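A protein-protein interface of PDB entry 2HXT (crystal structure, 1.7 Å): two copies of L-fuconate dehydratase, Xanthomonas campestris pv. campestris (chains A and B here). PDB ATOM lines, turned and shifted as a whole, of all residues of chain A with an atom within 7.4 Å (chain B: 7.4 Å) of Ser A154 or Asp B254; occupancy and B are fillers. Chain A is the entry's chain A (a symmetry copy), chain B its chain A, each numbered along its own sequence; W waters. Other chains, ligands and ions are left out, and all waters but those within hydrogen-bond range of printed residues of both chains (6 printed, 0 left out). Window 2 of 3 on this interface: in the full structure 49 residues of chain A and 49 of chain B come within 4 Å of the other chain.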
ATOM      1  N   PHE A 150     -15.144  17.237  25.473  1.00  0.00           N
ATOM      2  CA  PHE A 150     -15.204  17.829  26.802  1.00  0.00           C
ATOM      3  C   PHE A 150     -14.734  19.271  26.895  1.00  0.00           C
ATOM      4  O   PHE A 150     -14.748  19.861  27.978  1.00  0.00           O
ATOM      5  CB  PHE A 150     -14.435  16.958  27.802  1.00  0.00           C
ATOM      6  CG  PHE A 150     -15.121  15.657  28.112  1.00  0.00           C
ATOM      7  CD1 PHE A 150     -14.785  14.494  27.428  1.00  0.00           C
ATOM      8  CD2 PHE A 150     -16.145  15.609  29.056  1.00  0.00           C
ATOM      9  CE1 PHE A 150     -15.461  13.296  27.677  1.00  0.00           C
ATOM     10  CE2 PHE A 150     -16.828  14.419  29.314  1.00  0.00           C
ATOM     11  CZ  PHE A 150     -16.485  13.259  28.621  1.00  0.00           C
ATOM     12  N   ARG A 151     -14.325  19.849  25.771  1.00  0.00           N
ATOM     13  CA  ARG A 151     -13.885  21.238  25.788  1.00  0.00           C
ATOM     14  C   ARG A 151     -15.052  22.132  26.196  1.00  0.00           C
ATOM     15  O   ARG A 151     -16.197  21.886  25.808  1.00  0.00           O
ATOM     16  CB  ARG A 151     -13.361  21.664  24.412  1.00  0.00           C
ATOM     17  CG  ARG A 151     -12.928  23.129  24.363  1.00  0.00           C
ATOM     18  CD  ARG A 151     -12.062  23.422  23.146  1.00  0.00           C
ATOM     19  NE  ARG A 151     -12.762  23.173  21.891  1.00  0.00           N
ATOM     20  CZ  ARG A 151     -12.182  23.221  20.696  1.00  0.00           C
ATOM     21  NH1 ARG A 151     -10.891  23.509  20.597  1.00  0.00           N
ATOM     22  NH2 ARG A 151     -12.889  22.974  19.601  1.00  0.00           N
ATOM     23  N   TYR A 152     -14.743  23.155  26.990  1.00  0.00           N
ATOM     24  CA  TYR A 152     -15.714  24.124  27.495  1.00  0.00           C
ATOM     25  C   TYR A 152     -16.671  23.552  28.539  1.00  0.00           C
ATOM     26  O   TYR A 152     -17.630  24.216  28.936  1.00  0.00           O
ATOM     27  CB  TYR A 152     -16.521  24.735  26.341  1.00  0.00           C
ATOM     28  CG  TYR A 152     -15.668  25.330  25.242  1.00  0.00           C
ATOM     29  CD1 TYR A 152     -14.587  26.167  25.537  1.00  0.00           C
ATOM     30  CD2 TYR A 152     -15.944  25.059  23.905  1.00  0.00           C
ATOM     31  CE1 TYR A 152     -13.804  26.717  24.519  1.00  0.00           C
ATOM     32  CE2 TYR A 152     -15.171  25.600  22.881  1.00  0.00           C
ATOM     33  CZ  TYR A 152     -14.104  26.427  23.195  1.00  0.00           C
ATOM     34  OH  TYR A 152     -13.346  26.962  22.178  1.00  0.00           O
ATOM     35  N   LEU A 153     -16.403  22.331  28.998  1.00  0.00           N
ATOM     36  CA  LEU A 153     -17.266  21.702  29.997  1.00  0.00           C
ATOM     37  C   LEU A 153     -16.559  21.303  31.288  1.00  0.00           C
ATOM     38  O   LEU A 153     -17.201  20.783  32.199  1.00  0.00           O
ATOM     39  CB  LEU A 153     -17.927  20.449  29.412  1.00  0.00           C
ATOM     40  CG  LEU A 153     -18.856  20.607  28.208  1.00  0.00           C
ATOM     41  CD1 LEU A 153     -19.430  19.246  27.836  1.00  0.00           C
ATOM     42  CD2 LEU A 153     -19.976  21.581  28.541  1.00  0.00           C
ATOM     43  N   SER A 154     -15.254  21.549  31.385  1.00  0.00           N
ATOM     44  CA  SER A 154     -14.524  21.132  32.580  1.00  0.00           C
ATOM     45  C   SER A 154     -15.049  21.718  33.887  1.00  0.00           C
ATOM     46  O   SER A 154     -14.761  21.190  34.962  1.00  0.00           O
ATOM     47  CB  SER A 154     -13.025  21.431  32.432  1.00  0.00           C
ATOM     48  OG  SER A 154     -12.770  22.819  32.364  1.00  0.00           O
ATOM     49  N   ASP A 155     -15.822  22.794  33.800  1.00  0.00           N
ATOM     50  CA  ASP A 155     -16.386  23.415  34.995  1.00  0.00           C
ATOM     51  C   ASP A 155     -17.727  22.797  35.383  1.00  0.00           C
ATOM     52  O   ASP A 155     -18.269  23.098  36.450  1.00  0.00           O
ATOM     53  CB  ASP A 155     -16.563  24.929  34.787  1.00  0.00           C
ATOM     54  CG  ASP A 155     -17.272  25.272  33.481  1.00  0.00           C
ATOM     55  OD1 ASP A 155     -18.179  26.136  33.507  1.00  0.00           O
ATOM     56  OD2 ASP A 155     -16.917  24.699  32.426  1.00  0.00           O
ATOM     57  N   ALA A 156     -18.250  21.923  34.528  1.00  0.00           N
ATOM     58  CA  ALA A 156     -19.544  21.294  34.783  1.00  0.00           C
ATOM     59  C   ALA A 156     -19.578  19.777  34.615  1.00  0.00           C
ATOM     60  O   ALA A 156     -20.302  19.093  35.335  1.00  0.00           O
ATOM     61  CB  ALA A 156     -20.601  21.929  33.890  1.00  0.00           C
ATOM     62  N   LEU A 157     -18.813  19.252  33.660  1.00  0.00           N
ATOM     63  CA  LEU A 157     -18.777  17.811  33.414  1.00  0.00           C
ATOM     64  C   LEU A 157     -17.427  17.372  32.865  1.00  0.00           C
ATOM     65  O   LEU A 157     -17.103  17.656  31.711  1.00  0.00           O
ATOM     66  CB  LEU A 157     -19.859  17.413  32.407  1.00  0.00           C
ATOM     67  CG  LEU A 157     -19.895  15.933  32.018  1.00  0.00           C
ATOM     68  CD1 LEU A 157     -20.503  15.128  33.158  1.00  0.00           C
ATOM     69  CD2 LEU A 157     -20.715  15.748  30.744  1.00  0.00           C
ATOM     70  N   THR A 158     -16.645  16.679  33.683  1.00  0.00           N
ATOM     71  CA  THR A 158     -15.342  16.199  33.239  1.00  0.00           C
ATOM     72  C   THR A 158     -15.472  14.766  32.741  1.00  0.00           C
ATOM     73  O   THR A 158     -16.502  14.118  32.942  1.00  0.00           O
ATOM     74  CB  THR A 158     -14.310  16.210  34.378  1.00  0.00           C
ATOM     75  OG1 THR A 158     -14.691  15.252  35.373  1.00  0.00           O
ATOM     76  CG2 THR A 158     -14.217  17.593  35.004  1.00  0.00           C
ATOM     77  N   ARG A 159     -14.424  14.272  32.091  1.00  0.00           N
ATOM     78  CA  ARG A 159     -14.433  12.904  31.585  1.00  0.00           C
ATOM     79  C   ARG A 159     -14.640  11.932  32.745  1.00  0.00           C
ATOM     80  O   ARG A 159     -15.417  10.985  32.639  1.00  0.00           O
ATOM     81  CB  ARG A 159     -13.113  12.586  30.876  1.00  0.00           C
ATOM     82  CG  ARG A 159     -13.021  11.153  30.349  1.00  0.00           C
ATOM     83  CD  ARG A 159     -11.583  10.793  29.977  1.00  0.00           C
ATOM     84  NE  ARG A 159     -11.437   9.381  29.616  1.00  0.00           N
ATOM     85  CZ  ARG A 159     -11.660   8.890  28.402  1.00  0.00           C
ATOM     86  NH1 ARG A 159     -12.035   9.692  27.415  1.00  0.00           N
ATOM     87  NH2 ARG A 159     -11.515   7.591  28.177  1.00  0.00           N
ATOM     88  N   GLU A 161     -16.106  12.510  35.588  1.00  0.00           N
ATOM     89  CA  GLU A 161     -17.463  12.632  36.108  1.00  0.00           C
ATOM     90  C   GLU A 161     -18.456  11.905  35.202  1.00  0.00           C
ATOM     91  O   GLU A 161     -19.386  11.262  35.682  1.00  0.00           O
ATOM     92  CB  GLU A 161     -17.827  14.114  36.270  1.00  0.00           C
ATOM     93  CG  GLU A 161     -17.100  14.748  37.462  1.00  0.00           C
ATOM     94  CD  GLU A 161     -17.126  16.266  37.473  1.00  0.00           C
ATOM     95  OE1 GLU A 161     -16.674  16.849  38.485  1.00  0.00           O
ATOM     96  OE2 GLU A 161     -17.580  16.876  36.482  1.00  0.00           O
ATOM     97  N   LYS A 310     -25.038  23.892  28.913  1.00  0.00           N
ATOM     98  CA  LYS A 310     -24.341  23.949  30.197  1.00  0.00           C
ATOM     99  C   LYS A 310     -24.793  25.186  30.966  1.00  0.00           C
ATOM    100  O   LYS A 310     -25.113  25.111  32.149  1.00  0.00           O
ATOM    101  CB  LYS A 310     -22.821  24.009  30.002  1.00  0.00           C
ATOM    102  CG  LYS A 310     -22.052  24.111  31.323  1.00  0.00           C
ATOM    103  CD  LYS A 310     -20.566  24.384  31.121  1.00  0.00           C
ATOM    104  CE  LYS A 310     -20.320  25.765  30.525  1.00  0.00           C
ATOM    105  NZ  LYS A 310     -18.879  26.150  30.624  1.00  0.00           N
ATOM    106  N   GLN B 251     -10.448  31.714  21.711  1.00  0.00           N
ATOM    107  CA  GLN B 251     -11.366  30.724  22.292  1.00  0.00           C
ATOM    108  C   GLN B 251     -10.796  29.388  22.770  1.00  0.00           C
ATOM    109  O   GLN B 251     -11.554  28.479  23.092  1.00  0.00           O
ATOM    110  CB  GLN B 251     -12.480  30.432  21.277  1.00  0.00           C
ATOM    111  CG  GLN B 251     -12.993  31.666  20.538  1.00  0.00           C
ATOM    112  CD  GLN B 251     -13.760  31.311  19.274  1.00  0.00           C
ATOM    113  OE1 GLN B 251     -13.776  30.157  18.847  1.00  0.00           O
ATOM    114  NE2 GLN B 251     -14.391  32.308  18.666  1.00  0.00           N
ATOM    115  N   ARG B 252      -9.480  29.270  22.857  1.00  0.00           N
ATOM    116  CA  ARG B 252      -8.869  27.994  23.230  1.00  0.00           C
ATOM    117  C   ARG B 252      -9.114  27.375  24.601  1.00  0.00           C
ATOM    118  O   ARG B 252      -9.218  26.153  24.715  1.00  0.00           O
ATOM    119  CB  ARG B 252      -7.353  28.072  23.024  1.00  0.00           C
ATOM    120  CG  ARG B 252      -6.921  28.235  21.575  1.00  0.00           C
ATOM    121  CD  ARG B 252      -7.250  27.002  20.742  1.00  0.00           C
ATOM    122  NE  ARG B 252      -6.443  25.844  21.113  1.00  0.00           N
ATOM    123  CZ  ARG B 252      -6.461  24.688  20.457  1.00  0.00           C
ATOM    124  NH1 ARG B 252      -7.245  24.537  19.396  1.00  0.00           N
ATOM    125  NH2 ARG B 252      -5.693  23.684  20.857  1.00  0.00           N
ATOM    126  N   TRP B 253      -9.214  28.201  25.633  1.00  0.00           N
ATOM    127  CA  TRP B 253      -9.326  27.687  26.996  1.00  0.00           C
ATOM    128  C   TRP B 253     -10.684  27.466  27.639  1.00  0.00           C
ATOM    129  O   TRP B 253     -11.700  28.013  27.207  1.00  0.00           O
ATOM    130  CB  TRP B 253      -8.530  28.597  27.937  1.00  0.00           C
ATOM    131  CG  TRP B 253      -7.193  29.042  27.411  1.00  0.00           C
ATOM    132  CD1 TRP B 253      -6.232  28.261  26.835  1.00  0.00           C
ATOM    133  CD2 TRP B 253      -6.642  30.365  27.484  1.00  0.00           C
ATOM    134  NE1 TRP B 253      -5.115  29.013  26.549  1.00  0.00           N
ATOM    135  CE2 TRP B 253      -5.340  30.308  26.937  1.00  0.00           C
ATOM    136  CE3 TRP B 253      -7.123  31.592  27.963  1.00  0.00           C
ATOM    137  CZ2 TRP B 253      -4.510  31.430  26.856  1.00  0.00           C
ATOM    138  CZ3 TRP B 253      -6.295  32.711  27.883  1.00  0.00           C
ATOM    139  CH2 TRP B 253      -5.001  32.620  27.333  1.00  0.00           C
ATOM    140  N   ASP B 254     -10.669  26.640  28.686  1.00  0.00           N
ATOM    141  CA  ASP B 254     -11.848  26.380  29.506  1.00  0.00           C
ATOM    142  C   ASP B 254     -11.697  27.426  30.616  1.00  0.00           C
ATOM    143  O   ASP B 254     -10.656  28.082  30.706  1.00  0.00           O
ATOM    144  CB  ASP B 254     -11.820  24.971  30.120  1.00  0.00           C
ATOM    145  CG  ASP B 254     -12.389  23.908  29.192  1.00  0.00           C
ATOM    146  OD1 ASP B 254     -12.897  22.888  29.711  1.00  0.00           O
ATOM    147  OD2 ASP B 254     -12.325  24.077  27.957  1.00  0.00           O
ATOM    148  N   VAL B 255     -12.713  27.577  31.461  1.00  0.00           N
ATOM    149  CA  VAL B 255     -12.675  28.568  32.537  1.00  0.00           C
ATOM    150  C   VAL B 255     -11.484  28.464  33.499  1.00  0.00           C
ATOM    151  O   VAL B 255     -10.719  29.420  33.655  1.00  0.00           O
ATOM    152  CB  VAL B 255     -13.985  28.525  33.358  1.00  0.00           C
ATOM    153  CG1 VAL B 255     -13.881  29.449  34.569  1.00  0.00           C
ATOM    154  CG2 VAL B 255     -15.156  28.941  32.477  1.00  0.00           C
ATOM    155  N   GLY B 256     -11.336  27.314  34.151  1.00  0.00           N
ATOM    156  CA  GLY B 256     -10.236  27.136  35.086  1.00  0.00           C
ATOM    157  C   GLY B 256      -8.876  27.346  34.441  1.00  0.00           C
ATOM    158  O   GLY B 256      -8.063  28.127  34.940  1.00  0.00           O
ATOM    159  N   PRO B 257      -8.591  26.656  33.327  1.00  0.00           N
ATOM    160  CA  PRO B 257      -7.310  26.785  32.625  1.00  0.00           C
ATOM    161  C   PRO B 257      -7.000  28.213  32.167  1.00  0.00           C
ATOM    162  O   PRO B 257      -5.843  28.636  32.173  1.00  0.00           O
ATOM    163  CB  PRO B 257      -7.466  25.819  31.454  1.00  0.00           C
ATOM    164  CG  PRO B 257      -8.311  24.738  32.047  1.00  0.00           C
ATOM    165  CD  PRO B 257      -9.373  25.533  32.779  1.00  0.00           C
ATOM    166  N   ALA B 258      -8.034  28.952  31.771  1.00  0.00           N
ATOM    167  CA  ALA B 258      -7.848  30.331  31.319  1.00  0.00           C
ATOM    168  C   ALA B 258      -7.290  31.183  32.460  1.00  0.00           C
ATOM    169  O   ALA B 258      -6.356  31.966  32.273  1.00  0.00           O
ATOM    170  CB  ALA B 258      -9.174  30.909  30.837  1.00  0.00           C
ATOM    171  N   ILE B 259      -7.870  31.034  33.644  1.00  0.00           N
ATOM    172  CA  ILE B 259      -7.414  31.792  34.803  1.00  0.00           C
ATOM    173  C   ILE B 259      -5.961  31.446  35.142  1.00  0.00           C
ATOM    174  O   ILE B 259      -5.153  32.335  35.410  1.00  0.00           O
ATOM    175  CB  ILE B 259      -8.319  31.521  36.023  1.00  0.00           C
ATOM    176  CG1 ILE B 259      -9.739  32.016  35.725  1.00  0.00           C
ATOM    177  CG2 ILE B 259      -7.758  32.215  37.265  1.00  0.00           C
ATOM    178  CD1 ILE B 259     -10.774  31.619  36.773  1.00  0.00           C
ATOM    179  N   ASP B 260      -5.627  30.158  35.114  1.00  0.00           N
ATOM    180  CA  ASP B 260      -4.265  29.724  35.417  1.00  0.00           C
ATOM    181  C   ASP B 260      -3.276  30.196  34.362  1.00  0.00           C
ATOM    182  O   ASP B 260      -2.141  30.554  34.676  1.00  0.00           O
ATOM    183  CB  ASP B 260      -4.178  28.198  35.509  1.00  0.00           C
ATOM    184  CG  ASP B 260      -4.953  27.637  36.678  1.00  0.00           C
ATOM    185  OD1 ASP B 260      -5.042  28.324  37.718  1.00  0.00           O
ATOM    186  OD2 ASP B 260      -5.457  26.498  36.563  1.00  0.00           O
ATOM    187  N   PRO B 276     -10.878  34.498  25.760  1.00  0.00           N
ATOM    188  CA  PRO B 276     -10.213  33.449  26.534  1.00  0.00           C
ATOM    189  C   PRO B 276     -10.922  32.096  26.408  1.00  0.00           C
ATOM    190  O   PRO B 276     -10.293  31.052  26.542  1.00  0.00           O
ATOM    191  CB  PRO B 276     -10.234  34.003  27.961  1.00  0.00           C
ATOM    192  CG  PRO B 276     -11.460  34.886  27.975  1.00  0.00           C
ATOM    193  CD  PRO B 276     -11.369  35.579  26.634  1.00  0.00           C
ATOM    194  N   THR B 277     -12.224  32.115  26.132  1.00  0.00           N
ATOM    195  CA  THR B 277     -12.975  30.867  26.006  1.00  0.00           C
ATOM    196  C   THR B 277     -14.021  30.927  24.885  1.00  0.00           C
ATOM    197  O   THR B 277     -14.011  31.851  24.064  1.00  0.00           O
ATOM    198  CB  THR B 277     -13.647  30.498  27.364  1.00  0.00           C
ATOM    199  OG1 THR B 277     -14.114  29.142  27.325  1.00  0.00           O
ATOM    200  CG2 THR B 277     -14.815  31.430  27.662  1.00  0.00           C
ATOM    201  N   SER B 278     -14.905  29.932  24.843  1.00  0.00           N
ATOM    202  CA  SER B 278     -15.955  29.850  23.826  1.00  0.00           C
ATOM    203  C   SER B 278     -16.725  31.155  23.669  1.00  0.00           C
ATOM    204  O   SER B 278     -17.081  31.794  24.659  1.00  0.00           O
ATOM    205  CB  SER B 278     -16.943  28.739  24.181  1.00  0.00           C
ATOM    206  OG  SER B 278     -18.107  28.828  23.374  1.00  0.00           O
ATOM    207  N   ASP B 281     -19.935  31.223  25.707  1.00  0.00           N
ATOM    208  CA  ASP B 281     -19.946  31.115  27.160  1.00  0.00           C
ATOM    209  C   ASP B 281     -19.934  32.451  27.888  1.00  0.00           C
ATOM    210  O   ASP B 281     -18.884  32.967  28.275  1.00  0.00           O
ATOM    211  CB  ASP B 281     -18.779  30.235  27.624  1.00  0.00           C
ATOM    212  CG  ASP B 281     -19.069  29.529  28.939  1.00  0.00           C
ATOM    213  OD1 ASP B 281     -18.334  28.578  29.277  1.00  0.00           O
ATOM    214  OD2 ASP B 281     -20.029  29.926  29.635  1.00  0.00           O
ATOM    215  N   GLY B 284     -19.142  31.828  31.491  1.00  0.00           N
ATOM    216  CA  GLY B 284     -17.736  31.465  31.553  1.00  0.00           C
ATOM    217  C   GLY B 284     -16.811  32.667  31.486  1.00  0.00           C
ATOM    218  O   GLY B 284     -15.831  32.749  32.231  1.00  0.00           O
ATOM    219  N   ILE B 288     -14.169  33.930  34.331  1.00  0.00           N
ATOM    220  CA  ILE B 288     -12.761  34.173  34.040  1.00  0.00           C
ATOM    221  C   ILE B 288     -12.406  35.593  34.464  1.00  0.00           C
ATOM    222  O   ILE B 288     -11.376  35.825  35.101  1.00  0.00           O
ATOM    223  CB  ILE B 288     -12.467  33.991  32.534  1.00  0.00           C
ATOM    224  CG1 ILE B 288     -12.639  32.517  32.151  1.00  0.00           C
ATOM    225  CG2 ILE B 288     -11.052  34.466  32.211  1.00  0.00           C
ATOM    226  CD1 ILE B 288     -12.658  32.261  30.652  1.00  0.00           C
HETATM  227  O   HOH W   1     -14.940  25.838  30.652  1.00  0.00           O
HETATM  228  O   HOH W   2     -11.754  20.542  28.845  1.00  0.00           O
HETATM  229  O   HOH W   3     -12.803  24.903  34.177  1.00  0.00           O
HETATM  230  O   HOH W   4     -20.202  28.688  32.152  1.00  0.00           O
HETATM  231  O   HOH W   5     -14.866  27.889  20.025  1.00  0.00           O
HETATM  232  O   HOH W   6      -8.889  24.339  22.681  1.00  0.00           O
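Hydrophobic or aromatic side chains of chain A within 4 Å of the printed part of chain B: Tyr A152. Printed residues of chain B that touch a printed residue of chain A: Gln B251, Arg B252, Trp B253, Asp B254, Thr B277, Ser B278 and Asp B281. Among the printed residues, Asp or Glu carboxylates within 4 Å of a Lys or Arg side-chain nitrogen of the other chain: Lys A310 with Asp B281.
No position is printed for both chains.
Ser A154 touches just one residue of chain B: Asp B254. Asp B254 touches just these residues of chain A: Phe A150 (3.9 Å), Arg A151 (3.8 Å), Tyr A152 (2.8 Å), Leu A153 (3.6 Å) and Ser A154 (2.7 Å). Printed residues of chain A within 4 Å of Trp B253: Tyr A152 (3.7 Å). Printed residues of chain B within 4 Å of Arg A151: Arg B252 and Asp B254. Of the printed residues of chain A, Arg B252 touches Arg A151 (3.97 Å). Printed residues of chain A within 4 Å of Thr B277: Tyr A152 (3.5 Å). Asp A155 touches none of the printed residues of chain B. Pro B276 touches none of the printed residues of chain A. The nearest residue of chain A that does not touch Asp B254 is Asp A155 (5.0 Å).
Among the printed residues, pairs that only touch across the chains: Phe A150 with Asp B254, Arg A151 with Arg B252, Arg A151 with Asp B254, Tyr A152 with Trp B253, Tyr A152 with Thr B277, Tyr A152 with Ser B278 and Leu A153 with Asp B254.
OG1 of Thr B277 is in hydrogen-bond range of O of Trp B253 (2.7 Å). OD1 of Asp A155 is in salt-bridge range of NZ of Lys A310. N of Trp B253 lies within hydrogen-bond range of O of Pro B276 (3.2 Å). O of Tyr A152 is in hydrogen-bond range of NZ of Lys A310 (2.9 Å). The backbone NH (N) of Gly B284 sits at hydrogen-bond distance from the side-chain carboxylate (OD2) of Asp B281 (2.8 Å).
Water W6 bridges the backbone carbonyl oxygen (O) of Arg B252 (2.7 Å) and the guanidinium group (NH1) of Arg A151 (3.0 Å). Water W2 lies within hydrogen-bond range of the side-chain carboxylate of Asp B254 (2.7 Å) and the backbone carbonyl oxygen of Phe A150 (3.2 Å). Water W3 lies within hydrogen-bond range of the side-chain hydroxyl of Ser A154 (2.8 Å) and the backbone NH of Gly B256 (2.8 Å). Water W5 lies within hydrogen-bond range of the side-chain amide oxygen (OE1) of Gln B251 and the side-chain hydroxyl (OH) of Tyr A152. Water W4 lies within hydrogen-bond range of OD2 of Asp B281, NZ of Lys A310 and N of Gly B284. Water W1 lies within hydrogen-bond range of the side-chain carboxylate (OD2) of Asp A155 (2.9 Å) and the backbone NH (N) of Val B255 (2.9 Å).
The side-chain carboxylate (OD2) of Asp B254 is in hydrogen-bond range of the backbone NH (N) of Tyr A152 (2.8 Å). The side-chain amino group of Lys A310 lies within salt-bridge range of the side-chain carboxylate of Asp B281 (2.8 Å). The side-chain carboxylate of Asp B254 sits at hydrogen-bond distance from the side-chain hydroxyl of Ser A154 (2.7 Å). The backbone carbonyl oxygen of Gln B251 is in hydrogen-bond range of the side-chain hydroxyl of Tyr A152.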
